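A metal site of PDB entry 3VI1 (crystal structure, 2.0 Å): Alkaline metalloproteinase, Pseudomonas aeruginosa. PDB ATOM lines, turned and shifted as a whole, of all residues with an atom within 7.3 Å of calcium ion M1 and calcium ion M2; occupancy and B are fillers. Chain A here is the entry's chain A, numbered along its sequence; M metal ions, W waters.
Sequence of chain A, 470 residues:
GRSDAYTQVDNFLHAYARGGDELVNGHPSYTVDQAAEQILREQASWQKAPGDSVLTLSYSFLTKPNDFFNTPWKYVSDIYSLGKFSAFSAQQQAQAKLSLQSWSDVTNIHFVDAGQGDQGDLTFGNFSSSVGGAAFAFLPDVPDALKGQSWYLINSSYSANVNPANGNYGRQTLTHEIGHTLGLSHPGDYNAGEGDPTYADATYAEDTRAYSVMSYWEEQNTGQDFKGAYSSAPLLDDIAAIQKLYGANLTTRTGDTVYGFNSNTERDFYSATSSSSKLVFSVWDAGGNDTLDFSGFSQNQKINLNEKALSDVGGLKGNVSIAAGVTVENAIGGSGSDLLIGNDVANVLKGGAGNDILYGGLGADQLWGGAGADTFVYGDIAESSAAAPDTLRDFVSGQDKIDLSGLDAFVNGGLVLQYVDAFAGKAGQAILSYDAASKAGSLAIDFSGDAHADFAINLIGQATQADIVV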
ATOM      1  N   LEU A 305     -18.867   3.194  -6.348  1.00  0.00           N
ATOM      2  CA  LEU A 305     -19.816   2.343  -5.616  1.00  0.00           C
ATOM      3  C   LEU A 305     -19.655   0.840  -5.848  1.00  0.00           C
ATOM      4  O   LEU A 305     -20.345   0.037  -5.209  1.00  0.00           O
ATOM      5  CB  LEU A 305     -21.265   2.782  -5.883  1.00  0.00           C
ATOM      6  CG  LEU A 305     -21.771   4.072  -5.220  1.00  0.00           C
ATOM      7  CD1 LEU A 305     -23.248   4.270  -5.505  1.00  0.00           C
ATOM      8  CD2 LEU A 305     -21.529   4.089  -3.708  1.00  0.00           C
ATOM      9  N   GLU A 329     -25.671   1.186  -2.362  1.00  0.00           N
ATOM     10  CA  GLU A 329     -26.604   1.651  -3.381  1.00  0.00           C
ATOM     11  C   GLU A 329     -26.419   3.106  -3.804  1.00  0.00           C
ATOM     12  O   GLU A 329     -26.463   3.415  -4.994  1.00  0.00           O
ATOM     13  CB  GLU A 329     -28.054   1.444  -2.914  1.00  0.00           C
ATOM     14  CG  GLU A 329     -28.527  -0.012  -2.947  1.00  0.00           C
ATOM     15  CD  GLU A 329     -27.871  -0.887  -1.895  1.00  0.00           C
ATOM     16  OE1 GLU A 329     -27.466  -0.376  -0.826  1.00  0.00           O
ATOM     17  OE2 GLU A 329     -27.764  -2.118  -2.114  1.00  0.00           O
ATOM     18  N   ILE A 341     -19.372   7.253  -9.642  1.00  0.00           N
ATOM     19  CA  ILE A 341     -19.539   6.024 -10.412  1.00  0.00           C
ATOM     20  C   ILE A 341     -20.399   5.018  -9.635  1.00  0.00           C
ATOM     21  O   ILE A 341     -20.072   4.646  -8.507  1.00  0.00           O
ATOM     22  CB  ILE A 341     -18.174   5.388 -10.809  1.00  0.00           C
ATOM     23  CG1 ILE A 341     -17.348   6.386 -11.638  1.00  0.00           C
ATOM     24  CG2 ILE A 341     -18.396   4.088 -11.586  1.00  0.00           C
ATOM     25  CD1 ILE A 341     -15.955   5.902 -12.014  1.00  0.00           C
ATOM     26  N   GLY A 342     -21.503   4.610 -10.259  1.00  0.00           N
ATOM     27  CA  GLY A 342     -22.401   3.610  -9.676  1.00  0.00           C
ATOM     28  C   GLY A 342     -21.949   2.187  -9.971  1.00  0.00           C
ATOM     29  O   GLY A 342     -20.920   1.975 -10.608  1.00  0.00           O
ATOM     30  N   ASN A 343     -22.732   1.232  -9.494  1.00  0.00           N
ATOM     31  CA  ASN A 343     -22.442  -0.191  -9.704  1.00  0.00           C
ATOM     32  C   ASN A 343     -23.533  -0.882 -10.531  1.00  0.00           C
ATOM     33  O   ASN A 343     -24.279  -0.210 -11.250  1.00  0.00           O
ATOM     34  CB  ASN A 343     -22.201  -0.904  -8.359  1.00  0.00           C
ATOM     35  CG  ASN A 343     -23.310  -0.658  -7.355  1.00  0.00           C
ATOM     36  OD1 ASN A 343     -24.480  -0.530  -7.714  1.00  0.00           O
ATOM     37  ND2 ASN A 343     -22.949  -0.601  -6.081  1.00  0.00           N
ATOM     38  N   ASP A 344     -23.629  -2.197 -10.403  1.00  0.00           N
ATOM     39  CA  ASP A 344     -24.529  -2.984 -11.245  1.00  0.00           C
ATOM     40  C   ASP A 344     -26.019  -2.853 -10.899  1.00  0.00           C
ATOM     41  O   ASP A 344     -26.874  -3.074 -11.763  1.00  0.00           O
ATOM     42  CB  ASP A 344     -24.096  -4.449 -11.289  1.00  0.00           C
ATOM     43  CG  ASP A 344     -22.879  -4.668 -12.162  1.00  0.00           C
ATOM     44  OD1 ASP A 344     -22.318  -3.676 -12.690  1.00  0.00           O
ATOM     45  OD2 ASP A 344     -22.464  -5.838 -12.343  1.00  0.00           O
ATOM     46  N   VAL A 345     -26.326  -2.505  -9.654  1.00  0.00           N
ATOM     47  CA  VAL A 345     -27.726  -2.362  -9.225  1.00  0.00           C
ATOM     48  C   VAL A 345     -28.231  -0.918  -9.378  1.00  0.00           C
ATOM     49  O   VAL A 345     -27.487  -0.038  -9.822  1.00  0.00           O
ATOM     50  CB  VAL A 345     -27.947  -2.865  -7.758  1.00  0.00           C
ATOM     51  CG1 VAL A 345     -27.577  -4.334  -7.621  1.00  0.00           C
ATOM     52  CG2 VAL A 345     -27.190  -2.011  -6.744  1.00  0.00           C
ATOM     53  N   ALA A 346     -29.496  -0.698  -9.034  1.00  0.00           N
ATOM     54  CA  ALA A 346     -30.111   0.621  -9.088  1.00  0.00           C
ATOM     55  C   ALA A 346     -29.440   1.559  -8.087  1.00  0.00           C
ATOM     56  O   ALA A 346     -29.382   1.267  -6.893  1.00  0.00           O
ATOM     57  CB  ALA A 346     -31.611   0.534  -8.824  1.00  0.00           C
ATOM     58  N   ASN A 347     -28.933   2.687  -8.588  1.00  0.00           N
ATOM     59  CA  ASN A 347     -28.235   3.660  -7.741  1.00  0.00           C
ATOM     60  C   ASN A 347     -28.894   5.033  -7.731  1.00  0.00           C
ATOM     61  O   ASN A 347     -29.368   5.516  -8.757  1.00  0.00           O
ATOM     62  CB  ASN A 347     -26.774   3.823  -8.210  1.00  0.00           C
ATOM     63  CG  ASN A 347     -26.000   2.514  -8.201  1.00  0.00           C
ATOM     64  OD1 ASN A 347     -25.444   2.121  -9.222  1.00  0.00           O
ATOM     65  ND2 ASN A 347     -25.952   1.847  -7.063  1.00  0.00           N
ATOM     66  N   VAL A 348     -28.915   5.654  -6.555  1.00  0.00           N
ATOM     67  CA  VAL A 348     -29.251   7.066  -6.441  1.00  0.00           C
ATOM     68  C   VAL A 348     -27.948   7.841  -6.312  1.00  0.00           C
ATOM     69  O   VAL A 348     -27.228   7.719  -5.321  1.00  0.00           O
ATOM     70  CB  VAL A 348     -30.182   7.364  -5.234  1.00  0.00           C
ATOM     71  CG1 VAL A 348     -30.507   8.860  -5.163  1.00  0.00           C
ATOM     72  CG2 VAL A 348     -31.477   6.556  -5.325  1.00  0.00           C
ATOM     73  N   LEU A 349     -27.630   8.618  -7.347  1.00  0.00           N
ATOM     74  CA  LEU A 349     -26.412   9.436  -7.343  1.00  0.00           C
ATOM     75  C   LEU A 349     -26.762  10.911  -7.298  1.00  0.00           C
ATOM     76  O   LEU A 349     -27.503  11.417  -8.148  1.00  0.00           O
ATOM     77  CB  LEU A 349     -25.542   9.125  -8.572  1.00  0.00           C
ATOM     78  CG  LEU A 349     -24.993   7.697  -8.772  1.00  0.00           C
ATOM     79  CD1 LEU A 349     -24.232   7.619 -10.084  1.00  0.00           C
ATOM     80  CD2 LEU A 349     -24.116   7.255  -7.608  1.00  0.00           C
ATOM     81  N   TYR A 359     -22.051   8.583 -13.489  1.00  0.00           N
ATOM     82  CA  TYR A 359     -22.053   7.356 -14.287  1.00  0.00           C
ATOM     83  C   TYR A 359     -22.825   6.281 -13.538  1.00  0.00           C
ATOM     84  O   TYR A 359     -22.288   5.628 -12.639  1.00  0.00           O
ATOM     85  CB  TYR A 359     -20.616   6.907 -14.568  1.00  0.00           C
ATOM     86  CG  TYR A 359     -20.484   5.767 -15.549  1.00  0.00           C
ATOM     87  CD1 TYR A 359     -20.366   4.448 -15.107  1.00  0.00           C
ATOM     88  CD2 TYR A 359     -20.445   6.016 -16.923  1.00  0.00           C
ATOM     89  CE1 TYR A 359     -20.241   3.400 -16.018  1.00  0.00           C
ATOM     90  CE2 TYR A 359     -20.311   4.973 -17.835  1.00  0.00           C
ATOM     91  CZ  TYR A 359     -20.212   3.673 -17.377  1.00  0.00           C
ATOM     92  OH  TYR A 359     -20.073   2.642 -18.284  1.00  0.00           O
ATOM     93  N   GLY A 360     -24.081   6.104 -13.917  1.00  0.00           N
ATOM     94  CA  GLY A 360     -24.971   5.167 -13.247  1.00  0.00           C
ATOM     95  C   GLY A 360     -24.546   3.709 -13.365  1.00  0.00           C
ATOM     96  O   GLY A 360     -24.734   2.927 -12.431  1.00  0.00           O
ATOM     97  N   GLY A 361     -23.960   3.353 -14.504  1.00  0.00           N
ATOM     98  CA  GLY A 361     -23.598   1.977 -14.795  1.00  0.00           C
ATOM     99  C   GLY A 361     -24.829   1.162 -15.129  1.00  0.00           C
ATOM    100  O   GLY A 361     -25.830   1.707 -15.588  1.00  0.00           O
ATOM    101  N   LEU A 362     -24.761  -0.152 -14.889  1.00  0.00           N
ATOM    102  CA  LEU A 362     -25.885  -1.039 -15.154  1.00  0.00           C
ATOM    103  C   LEU A 362     -27.048  -0.781 -14.185  1.00  0.00           C
ATOM    104  O   LEU A 362     -26.844  -0.265 -13.086  1.00  0.00           O
ATOM    105  CB  LEU A 362     -25.441  -2.511 -15.100  1.00  0.00           C
ATOM    106  CG  LEU A 362     -24.460  -2.984 -16.177  1.00  0.00           C
ATOM    107  CD1 LEU A 362     -23.725  -4.240 -15.723  1.00  0.00           C
ATOM    108  CD2 LEU A 362     -25.133  -3.211 -17.519  1.00  0.00           C
ATOM    109  N   GLY A 363     -28.254  -1.134 -14.610  1.00  0.00           N
ATOM    110  CA  GLY A 363     -29.467  -0.912 -13.817  1.00  0.00           C
ATOM    111  C   GLY A 363     -30.156   0.406 -14.139  1.00  0.00           C
ATOM    112  O   GLY A 363     -29.615   1.225 -14.886  1.00  0.00           O
ATOM    113  N   ALA A 364     -31.343   0.588 -13.583  1.00  0.00           N
ATOM    114  CA  ALA A 364     -32.091   1.845 -13.731  1.00  0.00           C
ATOM    115  C   ALA A 364     -31.739   2.772 -12.577  1.00  0.00           C
ATOM    116  O   ALA A 364     -32.141   2.549 -11.436  1.00  0.00           O
ATOM    117  CB  ALA A 364     -33.578   1.573 -13.783  1.00  0.00           C
ATOM    118  N   ASP A 365     -30.986   3.836 -12.885  1.00  0.00           N
ATOM    119  CA  ASP A 365     -30.445   4.724 -11.857  1.00  0.00           C
ATOM    120  C   ASP A 365     -31.180   6.059 -11.761  1.00  0.00           C
ATOM    121  O   ASP A 365     -31.672   6.581 -12.762  1.00  0.00           O
ATOM    122  CB  ASP A 365     -28.954   4.970 -12.097  1.00  0.00           C
ATOM    123  CG  ASP A 365     -28.170   3.687 -12.241  1.00  0.00           C
ATOM    124  OD1 ASP A 365     -27.954   2.976 -11.235  1.00  0.00           O
ATOM    125  OD2 ASP A 365     -27.746   3.387 -13.382  1.00  0.00           O
ATOM    126  N   GLN A 366     -31.243   6.588 -10.548  1.00  0.00           N
ATOM    127  CA  GLN A 366     -31.813   7.906 -10.292  1.00  0.00           C
ATOM    128  C   GLN A 366     -30.674   8.904 -10.150  1.00  0.00           C
ATOM    129  O   GLN A 366     -29.920   8.869  -9.174  1.00  0.00           O
ATOM    130  CB  GLN A 366     -32.695   7.881  -9.041  1.00  0.00           C
ATOM    131  CG  GLN A 366     -33.678   6.708  -8.959  1.00  0.00           C
ATOM    132  CD  GLN A 366     -34.578   6.596 -10.184  1.00  0.00           C
ATOM    133  OE1 GLN A 366     -34.691   5.531 -10.796  1.00  0.00           O
ATOM    134  NE2 GLN A 366     -35.218   7.693 -10.561  1.00  0.00           N
ATOM    135  N   LEU A 367     -30.540   9.792 -11.130  1.00  0.00           N
ATOM    136  CA  LEU A 367     -29.383  10.676 -11.214  1.00  0.00           C
ATOM    137  C   LEU A 367     -29.715  12.142 -10.982  1.00  0.00           C
ATOM    138  O   LEU A 367     -30.435  12.773 -11.776  1.00  0.00           O
ATOM    139  CB  LEU A 367     -28.630  10.475 -12.537  1.00  0.00           C
ATOM    140  CG  LEU A 367     -28.237   9.045 -12.922  1.00  0.00           C
ATOM    141  CD1 LEU A 367     -27.465   9.037 -14.236  1.00  0.00           C
ATOM    142  CD2 LEU A 367     -27.422   8.354 -11.827  1.00  0.00           C
ATOM    143  N   VAL A 377     -23.052  10.338 -17.965  1.00  0.00           N
ATOM    144  CA  VAL A 377     -22.238   9.586 -18.920  1.00  0.00           C
ATOM    145  C   VAL A 377     -22.723   8.155 -19.100  1.00  0.00           C
ATOM    146  O   VAL A 377     -23.137   7.497 -18.138  1.00  0.00           O
ATOM    147  CB  VAL A 377     -20.734   9.601 -18.513  1.00  0.00           C
ATOM    148  CG1 VAL A 377     -19.886   8.718 -19.417  1.00  0.00           C
ATOM    149  CG2 VAL A 377     -20.192  11.024 -18.518  1.00  0.00           C
ATOM    150  N   TYR A 378     -22.675   7.676 -20.340  1.00  0.00           N
ATOM    151  CA  TYR A 378     -23.071   6.315 -20.687  1.00  0.00           C
ATOM    152  C   TYR A 378     -22.011   5.642 -21.553  1.00  0.00           C
ATOM    153  O   TYR A 378     -21.625   6.164 -22.598  1.00  0.00           O
ATOM    154  CB  TYR A 378     -24.450   6.326 -21.364  1.00  0.00           C
ATOM    155  CG  TYR A 378     -25.533   6.908 -20.490  1.00  0.00           C
ATOM    156  CD1 TYR A 378     -25.813   8.277 -20.508  1.00  0.00           C
ATOM    157  CD2 TYR A 378     -26.273   6.104 -19.626  1.00  0.00           C
ATOM    158  CE1 TYR A 378     -26.804   8.824 -19.692  1.00  0.00           C
ATOM    159  CE2 TYR A 378     -27.267   6.634 -18.807  1.00  0.00           C
ATOM    160  CZ  TYR A 378     -27.521   7.993 -18.849  1.00  0.00           C
ATOM    161  OH  TYR A 378     -28.505   8.523 -18.044  1.00  0.00           O
ATOM    162  N   ASP A 380     -22.252   2.118 -22.193  1.00  0.00           N
ATOM    163  CA  ASP A 380     -22.894   0.950 -22.795  1.00  0.00           C
ATOM    164  C   ASP A 380     -24.401   1.145 -22.899  1.00  0.00           C
ATOM    165  O   ASP A 380     -25.010   1.804 -22.053  1.00  0.00           O
ATOM    166  CB  ASP A 380     -22.576  -0.315 -21.982  1.00  0.00           C
ATOM    167  CG  ASP A 380     -22.768  -1.589 -22.779  1.00  0.00           C
ATOM    168  OD1 ASP A 380     -23.904  -1.879 -23.195  1.00  0.00           O
ATOM    169  OD2 ASP A 380     -21.764  -2.303 -22.986  1.00  0.00           O
ATOM    170  N   ALA A 382     -26.737  -1.152 -22.594  1.00  0.00           N
ATOM    171  CA  ALA A 382     -27.386  -1.932 -21.526  1.00  0.00           C
ATOM    172  C   ALA A 382     -27.509  -1.172 -20.203  1.00  0.00           C
ATOM    173  O   ALA A 382     -28.253  -1.577 -19.312  1.00  0.00           O
ATOM    174  CB  ALA A 382     -26.640  -3.248 -21.326  1.00  0.00           C
ATOM    175  N   GLU A 383     -26.768  -0.071 -20.082  1.00  0.00           N
ATOM    176  CA  GLU A 383     -26.775   0.754 -18.879  1.00  0.00           C
ATOM    177  C   GLU A 383     -28.087   1.525 -18.698  1.00  0.00           C
ATOM    178  O   GLU A 383     -28.439   1.905 -17.573  1.00  0.00           O
ATOM    179  CB  GLU A 383     -25.577   1.705 -18.861  1.00  0.00           C
ATOM    180  CG  GLU A 383     -24.252   0.993 -18.610  1.00  0.00           C
ATOM    181  CD  GLU A 383     -23.035   1.831 -18.956  1.00  0.00           C
ATOM    182  OE1 GLU A 383     -23.173   3.067 -19.143  1.00  0.00           O
ATOM    183  OE2 GLU A 383     -21.945   1.254 -19.040  1.00  0.00           O
ATOM    184  N   SER A 384     -28.804   1.766 -19.792  1.00  0.00           N
ATOM    185  CA  SER A 384     -30.118   2.386 -19.732  1.00  0.00           C
ATOM    186  C   SER A 384     -31.024   1.803 -20.819  1.00  0.00           C
ATOM    187  O   SER A 384     -31.147   2.356 -21.909  1.00  0.00           O
ATOM    188  CB  SER A 384     -30.001   3.910 -19.855  1.00  0.00           C
ATOM    189  OG  SER A 384     -31.113   4.559 -19.264  1.00  0.00           O
ATOM    190  N   SER A 385     -31.639   0.666 -20.498  1.00  0.00           N
ATOM    191  CA  SER A 385     -32.513  -0.052 -21.430  1.00  0.00           C
ATOM    192  C   SER A 385     -33.804   0.703 -21.704  1.00  0.00           C
ATOM    193  O   SER A 385     -34.226   1.545 -20.896  1.00  0.00           O
ATOM    194  CB  SER A 385     -32.831  -1.445 -20.877  1.00  0.00           C
ATOM    195  OG  SER A 385     -33.510  -1.362 -19.635  1.00  0.00           O
ATOM    196  N   ALA A 388     -36.296  -0.348 -18.894  1.00  0.00           N
ATOM    197  CA  ALA A 388     -35.952   0.098 -17.549  1.00  0.00           C
ATOM    198  C   ALA A 388     -34.852   1.175 -17.577  1.00  0.00           C
ATOM    199  O   ALA A 388     -33.707   0.918 -17.193  1.00  0.00           O
ATOM    200  CB  ALA A 388     -35.537  -1.084 -16.679  1.00  0.00           C
ATOM    201  N   PRO A 389     -35.202   2.397 -18.029  1.00  0.00           N
ATOM    202  CA  PRO A 389     -34.201   3.448 -18.224  1.00  0.00           C
ATOM    203  C   PRO A 389     -33.829   4.213 -16.960  1.00  0.00           C
ATOM    204  O   PRO A 389     -34.538   4.164 -15.950  1.00  0.00           O
ATOM    205  CB  PRO A 389     -34.892   4.381 -19.213  1.00  0.00           C
ATOM    206  CG  PRO A 389     -36.344   4.241 -18.933  1.00  0.00           C
ATOM    207  CD  PRO A 389     -36.552   2.851 -18.389  1.00  0.00           C
ATOM    208  N   ASP A 390     -32.694   4.916 -17.035  1.00  0.00           N
ATOM    209  CA  ASP A 390     -32.291   5.899 -16.032  1.00  0.00           C
ATOM    210  C   ASP A 390     -33.280   7.040 -15.987  1.00  0.00           C
ATOM    211  O   ASP A 390     -33.989   7.302 -16.969  1.00  0.00           O
ATOM    212  CB  ASP A 390     -30.921   6.489 -16.399  1.00  0.00           C
ATOM    213  CG  ASP A 390     -29.758   5.637 -15.923  1.00  0.00           C
ATOM    214  OD1 ASP A 390     -29.956   4.450 -15.571  1.00  0.00           O
ATOM    215  OD2 ASP A 390     -28.620   6.162 -15.913  1.00  0.00           O
HETATM  216 CA    CA M   1     -27.940   2.749 -15.532  1.00  0.00          CA
HETATM  217 CA    CA M   2     -26.106   1.230 -11.363  1.00  0.00          CA
HETATM  218  O   HOH W   1     -26.605   4.522 -16.110  1.00  0.00           O
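Water W1 lies within hydrogen-bond range of the side-chain carboxylate (OD2) of Asp 390 (2.6 Å) and the backbone NH (N) of Gly 361 (3.3 Å).
Seven residues have an atom within 4 Å of calcium ion M2: Asn 343, Val 345, Asn 347, Gly 360, Gly 361, Leu 362 and Asp 365.
Calcium ion M1 is bound by the side-chain carboxylate (OD2) of Asp 365, the backbone carbonyl oxygen (O) of Glu 383, water W1, the backbone carbonyl oxygen (O) of Gly 361, the backbone carbonyl oxygen (O) of Gly 363 and the side-chain carboxylate (OD1) of Asp 390. Calcium ion M1 has six donor atoms within binding distance.
O of Asn 343 binds calcium ion M2 (2.3 Å). O of Leu 362 is bound to calcium ion M2 (2.4 Å). The side-chain amide oxygen (OD1) of Asn 347 is bound to calcium ion M2 (2.4 Å). Calcium ion M2 is bound by O of Val 345 (2.4 Å). Calcium ion M2 is bound by O of Gly 360 (2.4 Å). OD1 of Asp 365 is bound to calcium ion M2 (2.5 Å). Calcium ion M2 has six donor atoms within binding distance.
Six residues have an atom within 4 Å of calcium ion M1: Gly 361, Leu 362, Gly 363, Asp 365, Glu 383 and Asp 390.
The side-chain carboxylate (OE2) of Glu 383 lies within hydrogen-bond range of the side-chain hydroxyl (OH) of Tyr 359 (2.4 Å). The backbone NH (N) of Asp 380 is in hydrogen-bond range of the side-chain carboxylate (OE2) of Glu 383. The backbone NH (N) of Val 345 sits close to the side-chain amide oxygen (OD1) of Asn 343 (3.3 Å). O of Leu 305 is in hydrogen-bond range of ND2 of Asn 343 (2.8 Å). The side-chain amide nitrogen (ND2) of Asn 347 lies within hydrogen-bond range of the backbone carbonyl oxygen (O) of Glu 329. O of Asn 347 sits at hydrogen-bond distance from N of Gln 366 (2.8 Å). N of Asp 390 sits at hydrogen-bond distance from OG of Ser 384. OD2 of Asp 390 sits at hydrogen-bond distance from OH of Tyr 378 (3.2 Å).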
